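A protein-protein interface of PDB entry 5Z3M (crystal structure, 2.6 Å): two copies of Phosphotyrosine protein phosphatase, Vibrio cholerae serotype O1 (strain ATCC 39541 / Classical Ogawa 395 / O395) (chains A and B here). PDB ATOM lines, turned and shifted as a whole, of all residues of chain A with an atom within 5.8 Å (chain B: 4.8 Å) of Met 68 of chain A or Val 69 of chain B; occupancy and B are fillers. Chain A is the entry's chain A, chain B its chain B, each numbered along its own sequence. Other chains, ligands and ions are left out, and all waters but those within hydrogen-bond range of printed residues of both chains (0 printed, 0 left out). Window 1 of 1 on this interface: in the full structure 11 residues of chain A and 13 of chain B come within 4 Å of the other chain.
O of Met 68 of chain A lies close to SD of Met 68 of chain B (3.1 Å).
The backbone NH (N) of Val 69 of chain B is in hydrogen-bond range of the backbone carbonyl oxygen (O) of Val 69 of chain A (3.0 Å).
The side-chain sulfur (SD) of Met 68 of chain B lies close to the side-chain amide nitrogen (ND2) of Asn 70 of chain A.
NE2 of His 66 of chain A sits close to ND2 of Asn 70 of chain B, at 3.5 Å.
Among the printed residues, merely in contact across the chains: Pro 67 of chain A with Pro 71 of chain B, Val 69 of chain A with Met 68 of chain B, Met 68 of chain A with Asn 70 of chain B, Met 51 of chain A with Pro 67 of chain B, Val 69 of chain A with Met 51 of chain B, Met 51 of chain A with Val 69 of chain B, Pro 67 of chain A with Asn 70 of chain B, Pro 67 of chain A with Val 69 of chain B, Met 51 of chain A with Leu 57 of chain B, Met 68 of chain A with Arg 27 of chain B and Met 68 of chain A with Val 69 of chain B.
Pro 67 of chain A touches Val 69 of chain B, but with the chains exchanged Val 69 of chain A does not touch Pro 67 of chain B (4.02 Å).
Met 68 of chain A touches Val 69 of chain B, and with the chains exchanged Val 69 of chain A touches Met 68 of chain B.
Met 68 of chain A touches Asn 70 of chain B, and with the chains exchanged Asn 70 of chain A touches Met 68 of chain B.
Val 69 of chain A touches its own counterpart, Val 69 of chain B.
Positions printed for both chains: 24, 27, 51, 67, 68, 69 and 70.
The guanidinium group of Arg 27 of chain B is in hydrogen-bond range of the side-chain amide oxygen of Asn 70 of chain B (2.9 Å).
OE2 of Glu 23 of chain B is in salt-bridge range of NH1 of Arg 27 of chain B (3.2 Å).
The side-chain carboxylate (OE2) of Glu 23 of chain B sits close to the side-chain amide oxygen (OD1) of Asn 70 of chain B, 2.8 Å away.
Ile 24 of chain A touches none of the printed residues of chain B.
Of the printed residues of chain B, Met 68 of chain A touches Arg 27 (3.9 Å), Met 68 (3.1 Å), Val 69 (3.99 Å) and Asn 70 (3.4 Å).
Of the printed residues of chain B, Asn 70 of chain A touches Met 68 (3.3 Å).
Printed residues of chain A within 4 Å of Arg 27 of chain B: Met 68.
Pro 52 of chain B touches none of the printed residues of chain A.
Of the printed residues of chain A, Met 68 of chain B touches Met 68, Val 69 and Asn 70.
Printed residues of chain A within 4 Å of Val 69 of chain B: Met 51, Pro 67, Met 68 and Val 69.
The nearest printed residue of chain B that does not touch Met 68 of chain A is Pro 71 of chain B (5.2 Å).
The nearest printed residue of chain A that does not touch Pro 67 of chain B is Val 69 of chain A (4.02 Å).
Hydrophobic or aromatic side chains of chain A that line the printed part of chain B: Met 51, His 66, Pro 67, Met 68 and Val 69.
Printed residues of chain B that touch a printed residue of chain A: Arg 27, Met 51, Leu 57, Pro 67, Met 68, Val 69, Asn 70 and Pro 71.
Hydrophobic or aromatic side chains of chain B that line the printed part of chain A: Met 51, Leu 57, Met 68, Val 69 and Pro 71.
Among the printed residues, 15 pairs touch across the chains.
Among the printed residues, no Asp or Glu carboxylate lies within 4 Å of a Lys or Arg side-chain nitrogen of the other chain.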
ATOM      1  N   ILE A  24     -13.947 -23.564   2.722  1.00  0.00           N
ATOM      2  CA  ILE A  24     -14.187 -22.126   2.728  1.00  0.00           C
ATOM      3  C   ILE A  24     -13.297 -21.437   3.762  1.00  0.00           C
ATOM      4  O   ILE A  24     -12.639 -20.439   3.456  1.00  0.00           O
ATOM      5  CB  ILE A  24     -15.666 -21.798   3.011  1.00  0.00           C
ATOM      6  CG1 ILE A  24     -16.528 -22.159   1.797  1.00  0.00           C
ATOM      7  CG2 ILE A  24     -15.829 -20.323   3.342  1.00  0.00           C
ATOM      8  CD1 ILE A  24     -17.858 -22.780   2.158  1.00  0.00           C
ATOM      9  N   ARG A  27      -9.752 -21.341   2.449  1.00  0.00           N
ATOM     10  CA  ARG A  27      -9.464 -20.405   1.365  1.00  0.00           C
ATOM     11  C   ARG A  27      -9.280 -18.981   1.881  1.00  0.00           C
ATOM     12  O   ARG A  27      -8.429 -18.244   1.386  1.00  0.00           O
ATOM     13  CB  ARG A  27     -10.569 -20.436   0.307  1.00  0.00           C
ATOM     14  CG  ARG A  27     -10.075 -20.106  -1.097  1.00  0.00           C
ATOM     15  CD  ARG A  27     -11.225 -19.934  -2.076  1.00  0.00           C
ATOM     16  NE  ARG A  27     -12.333 -20.837  -1.783  1.00  0.00           N
ATOM     17  CZ  ARG A  27     -12.403 -22.098  -2.192  1.00  0.00           C
ATOM     18  NH1 ARG A  27     -11.421 -22.621  -2.915  1.00  0.00           N
ATOM     19  NH2 ARG A  27     -13.455 -22.838  -1.875  1.00  0.00           N
ATOM     20  N   MET A  51     -25.560 -28.577  -4.032  1.00  0.00           N
ATOM     21  CA  MET A  51     -24.870 -27.614  -3.197  1.00  0.00           C
ATOM     22  C   MET A  51     -24.740 -28.125  -1.771  1.00  0.00           C
ATOM     23  O   MET A  51     -25.578 -28.896  -1.306  1.00  0.00           O
ATOM     24  CB  MET A  51     -25.618 -26.276  -3.212  1.00  0.00           C
ATOM     25  CG  MET A  51     -25.467 -25.502  -4.496  1.00  0.00           C
ATOM     26  SD  MET A  51     -23.824 -24.769  -4.629  1.00  0.00           S
ATOM     27  CE  MET A  51     -23.526 -24.941  -6.387  1.00  0.00           C
ATOM     28  N   HIS A  66     -18.065 -14.574   3.498  1.00  0.00           N
ATOM     29  CA  HIS A  66     -18.883 -14.385   2.320  1.00  0.00           C
ATOM     30  C   HIS A  66     -18.411 -15.380   1.277  1.00  0.00           C
ATOM     31  O   HIS A  66     -17.528 -15.069   0.482  1.00  0.00           O
ATOM     32  CB  HIS A  66     -18.761 -12.953   1.811  1.00  0.00           C
ATOM     33  CG  HIS A  66     -19.490 -12.711   0.526  1.00  0.00           C
ATOM     34  ND1 HIS A  66     -20.598 -13.434   0.154  1.00  0.00           N
ATOM     35  CD2 HIS A  66     -19.259 -11.824  -0.468  1.00  0.00           C
ATOM     36  CE1 HIS A  66     -21.030 -12.998  -1.021  1.00  0.00           C
ATOM     37  NE2 HIS A  66     -20.237 -12.026  -1.418  1.00  0.00           N
ATOM     38  N   PRO A  67     -18.987 -16.589   1.288  1.00  0.00           N
ATOM     39  CA  PRO A  67     -18.347 -17.678   0.549  1.00  0.00           C
ATOM     40  C   PRO A  67     -18.872 -17.905  -0.871  1.00  0.00           C
ATOM     41  O   PRO A  67     -20.071 -18.081  -1.077  1.00  0.00           O
ATOM     42  CB  PRO A  67     -18.641 -18.893   1.434  1.00  0.00           C
ATOM     43  CG  PRO A  67     -19.971 -18.562   2.065  1.00  0.00           C
ATOM     44  CD  PRO A  67     -20.095 -17.070   2.133  1.00  0.00           C
ATOM     45  N   MET A  68     -17.962 -17.872  -1.841  1.00  0.00           N
ATOM     46  CA  MET A  68     -18.231 -18.422  -3.162  1.00  0.00           C
ATOM     47  C   MET A  68     -18.105 -19.927  -3.031  1.00  0.00           C
ATOM     48  O   MET A  68     -16.990 -20.445  -2.994  1.00  0.00           O
ATOM     49  CB  MET A  68     -17.247 -17.890  -4.208  1.00  0.00           C
ATOM     50  CG  MET A  68     -17.791 -16.832  -5.166  1.00  0.00           C
ATOM     51  SD  MET A  68     -16.460 -16.212  -6.221  1.00  0.00           S
ATOM     52  CE  MET A  68     -15.153 -16.007  -5.005  1.00  0.00           C
ATOM     53  N   VAL A  69     -19.230 -20.636  -2.947  1.00  0.00           N
ATOM     54  CA  VAL A  69     -19.178 -22.075  -2.665  1.00  0.00           C
ATOM     55  C   VAL A  69     -19.203 -22.957  -3.919  1.00  0.00           C
ATOM     56  O   VAL A  69     -20.019 -22.774  -4.828  1.00  0.00           O
ATOM     57  CB  VAL A  69     -20.321 -22.500  -1.709  1.00  0.00           C
ATOM     58  CG1 VAL A  69     -21.360 -21.428  -1.612  1.00  0.00           C
ATOM     59  CG2 VAL A  69     -20.949 -23.827  -2.133  1.00  0.00           C
ATOM     60  N   ASN A  70     -18.277 -23.911  -3.939  1.00  0.00           N
ATOM     61  CA  ASN A  70     -18.186 -24.911  -4.985  1.00  0.00           C
ATOM     62  C   ASN A  70     -19.265 -25.973  -4.846  1.00  0.00           C
ATOM     63  O   ASN A  70     -19.615 -26.360  -3.732  1.00  0.00           O
ATOM     64  CB  ASN A  70     -16.813 -25.582  -4.963  1.00  0.00           C
ATOM     65  CG  ASN A  70     -15.746 -24.750  -5.638  1.00  0.00           C
ATOM     66  OD1 ASN A  70     -14.622 -24.644  -5.151  1.00  0.00           O
ATOM     67  ND2 ASN A  70     -16.090 -24.160  -6.770  1.00  0.00           N
ATOM     68  N   GLU B  23     -24.633 -13.968 -12.678  1.00  0.00           N
ATOM     69  CA  GLU B  23     -23.445 -13.748 -11.864  1.00  0.00           C
ATOM     70  C   GLU B  23     -22.308 -14.681 -12.287  1.00  0.00           C
ATOM     71  O   GLU B  23     -21.161 -14.248 -12.410  1.00  0.00           O
ATOM     72  CB  GLU B  23     -23.779 -13.942 -10.380  1.00  0.00           C
ATOM     73  CG  GLU B  23     -22.785 -13.310  -9.413  1.00  0.00           C
ATOM     74  CD  GLU B  23     -22.776 -13.987  -8.055  1.00  0.00           C
ATOM     75  OE1 GLU B  23     -23.686 -14.799  -7.791  1.00  0.00           O
ATOM     76  OE2 GLU B  23     -21.852 -13.719  -7.258  1.00  0.00           O
ATOM     77  N   ILE B  24     -22.632 -15.952 -12.511  1.00  0.00           N
ATOM     78  CA  ILE B  24     -21.670 -16.937 -13.008  1.00  0.00           C
ATOM     79  C   ILE B  24     -21.142 -16.575 -14.402  1.00  0.00           C
ATOM     80  O   ILE B  24     -19.930 -16.480 -14.612  1.00  0.00           O
ATOM     81  CB  ILE B  24     -22.301 -18.353 -13.060  1.00  0.00           C
ATOM     82  CG1 ILE B  24     -22.899 -18.730 -11.701  1.00  0.00           C
ATOM     83  CG2 ILE B  24     -21.280 -19.392 -13.512  1.00  0.00           C
ATOM     84  CD1 ILE B  24     -24.169 -19.539 -11.786  1.00  0.00           C
ATOM     85  N   ARG B  27     -18.767 -13.714 -14.617  1.00  0.00           N
ATOM     86  CA  ARG B  27     -17.457 -14.167 -14.138  1.00  0.00           C
ATOM     87  C   ARG B  27     -16.677 -14.935 -15.192  1.00  0.00           C
ATOM     88  O   ARG B  27     -15.492 -14.684 -15.392  1.00  0.00           O
ATOM     89  CB  ARG B  27     -17.611 -15.035 -12.891  1.00  0.00           C
ATOM     90  CG  ARG B  27     -17.165 -14.349 -11.632  1.00  0.00           C
ATOM     91  CD  ARG B  27     -17.712 -15.048 -10.422  1.00  0.00           C
ATOM     92  NE  ARG B  27     -18.237 -14.090  -9.462  1.00  0.00           N
ATOM     93  CZ  ARG B  27     -19.130 -14.391  -8.529  1.00  0.00           C
ATOM     94  NH1 ARG B  27     -19.595 -15.627  -8.432  1.00  0.00           N
ATOM     95  NH2 ARG B  27     -19.559 -13.458  -7.695  1.00  0.00           N
ATOM     96  N   MET B  51     -29.132 -20.945  -0.687  1.00  0.00           N
ATOM     97  CA  MET B  51     -28.543 -21.185  -1.993  1.00  0.00           C
ATOM     98  C   MET B  51     -29.547 -21.007  -3.125  1.00  0.00           C
ATOM     99  O   MET B  51     -30.727 -21.339  -2.981  1.00  0.00           O
ATOM    100  CB  MET B  51     -27.933 -22.588  -2.043  1.00  0.00           C
ATOM    101  CG  MET B  51     -26.689 -22.721  -1.193  1.00  0.00           C
ATOM    102  SD  MET B  51     -25.428 -21.564  -1.767  1.00  0.00           S
ATOM    103  CE  MET B  51     -24.594 -21.190  -0.226  1.00  0.00           C
ATOM    104  N   PRO B  52     -29.077 -20.451  -4.250  1.00  0.00           N
ATOM    105  CA  PRO B  52     -29.834 -20.407  -5.505  1.00  0.00           C
ATOM    106  C   PRO B  52     -30.423 -21.776  -5.826  1.00  0.00           C
ATOM    107  O   PRO B  52     -29.810 -22.783  -5.462  1.00  0.00           O
ATOM    108  CB  PRO B  52     -28.776 -20.008  -6.532  1.00  0.00           C
ATOM    109  CG  PRO B  52     -27.806 -19.185  -5.760  1.00  0.00           C
ATOM    110  CD  PRO B  52     -27.789 -19.741  -4.355  1.00  0.00           C
ATOM    111  N   LEU B  57     -28.759 -23.857 -11.254  1.00  0.00           N
ATOM    112  CA  LEU B  57     -27.332 -24.182 -11.224  1.00  0.00           C
ATOM    113  C   LEU B  57     -26.940 -25.179 -12.312  1.00  0.00           C
ATOM    114  O   LEU B  57     -25.887 -25.048 -12.937  1.00  0.00           O
ATOM    115  CB  LEU B  57     -26.947 -24.736  -9.850  1.00  0.00           C
ATOM    116  CG  LEU B  57     -26.964 -23.707  -8.721  1.00  0.00           C
ATOM    117  CD1 LEU B  57     -27.277 -24.352  -7.384  1.00  0.00           C
ATOM    118  CD2 LEU B  57     -25.637 -22.982  -8.656  1.00  0.00           C
ATOM    119  N   PRO B  67     -20.643 -23.470 -11.600  1.00  0.00           N
ATOM    120  CA  PRO B  67     -21.487 -22.563 -10.823  1.00  0.00           C
ATOM    121  C   PRO B  67     -21.027 -22.420  -9.378  1.00  0.00           C
ATOM    122  O   PRO B  67     -21.724 -22.863  -8.468  1.00  0.00           O
ATOM    123  CB  PRO B  67     -22.856 -23.233 -10.897  1.00  0.00           C
ATOM    124  CG  PRO B  67     -22.530 -24.699 -10.964  1.00  0.00           C
ATOM    125  CD  PRO B  67     -21.177 -24.843 -11.598  1.00  0.00           C
ATOM    126  N   MET B  68     -19.854 -21.829  -9.179  1.00  0.00           N
ATOM    127  CA  MET B  68     -19.329 -21.590  -7.840  1.00  0.00           C
ATOM    128  C   MET B  68     -19.956 -20.282  -7.331  1.00  0.00           C
ATOM    129  O   MET B  68     -19.618 -19.185  -7.783  1.00  0.00           O
ATOM    130  CB  MET B  68     -17.782 -21.601  -7.877  1.00  0.00           C
ATOM    131  CG  MET B  68     -17.011 -20.380  -7.378  1.00  0.00           C
ATOM    132  SD  MET B  68     -16.010 -20.792  -5.933  1.00  0.00           S
ATOM    133  CE  MET B  68     -14.571 -19.740  -6.145  1.00  0.00           C
ATOM    134  N   VAL B  69     -20.913 -20.417  -6.411  1.00  0.00           N
ATOM    135  CA  VAL B  69     -21.901 -19.353  -6.173  1.00  0.00           C
ATOM    136  C   VAL B  69     -21.920 -18.698  -4.791  1.00  0.00           C
ATOM    137  O   VAL B  69     -22.059 -19.379  -3.778  1.00  0.00           O
ATOM    138  CB  VAL B  69     -23.332 -19.878  -6.418  1.00  0.00           C
ATOM    139  CG1 VAL B  69     -23.833 -19.471  -7.793  1.00  0.00           C
ATOM    140  CG2 VAL B  69     -23.392 -21.385  -6.220  1.00  0.00           C
ATOM    141  N   ASN B  70     -21.821 -17.369  -4.773  1.00  0.00           N
ATOM    142  CA  ASN B  70     -22.139 -16.591  -3.583  1.00  0.00           C
ATOM    143  C   ASN B  70     -23.556 -16.935  -3.151  1.00  0.00           C
ATOM    144  O   ASN B  70     -24.404 -17.200  -4.002  1.00  0.00           O
ATOM    145  CB  ASN B  70     -22.019 -15.085  -3.852  1.00  0.00           C
ATOM    146  CG  ASN B  70     -20.583 -14.625  -3.997  1.00  0.00           C
ATOM    147  OD1 ASN B  70     -20.237 -13.918  -4.940  1.00  0.00           O
ATOM    148  ND2 ASN B  70     -19.741 -15.022  -3.057  1.00  0.00           N
ATOM    149  N   PRO B  71     -23.820 -16.959  -1.833  1.00  0.00           N
ATOM    150  CA  PRO B  71     -25.186 -17.243  -1.388  1.00  0.00           C
ATOM    151  C   PRO B  71     -26.118 -16.058  -1.588  1.00  0.00           C
ATOM    152  O   PRO B  71     -25.679 -14.944  -1.891  1.00  0.00           O
ATOM    153  CB  PRO B  71     -25.030 -17.574   0.105  1.00  0.00           C
ATOM    154  CG  PRO B  71     -23.645 -17.180   0.481  1.00  0.00           C
ATOM    155  CD  PRO B  71     -22.919 -16.657  -0.710  1.00  0.00           C
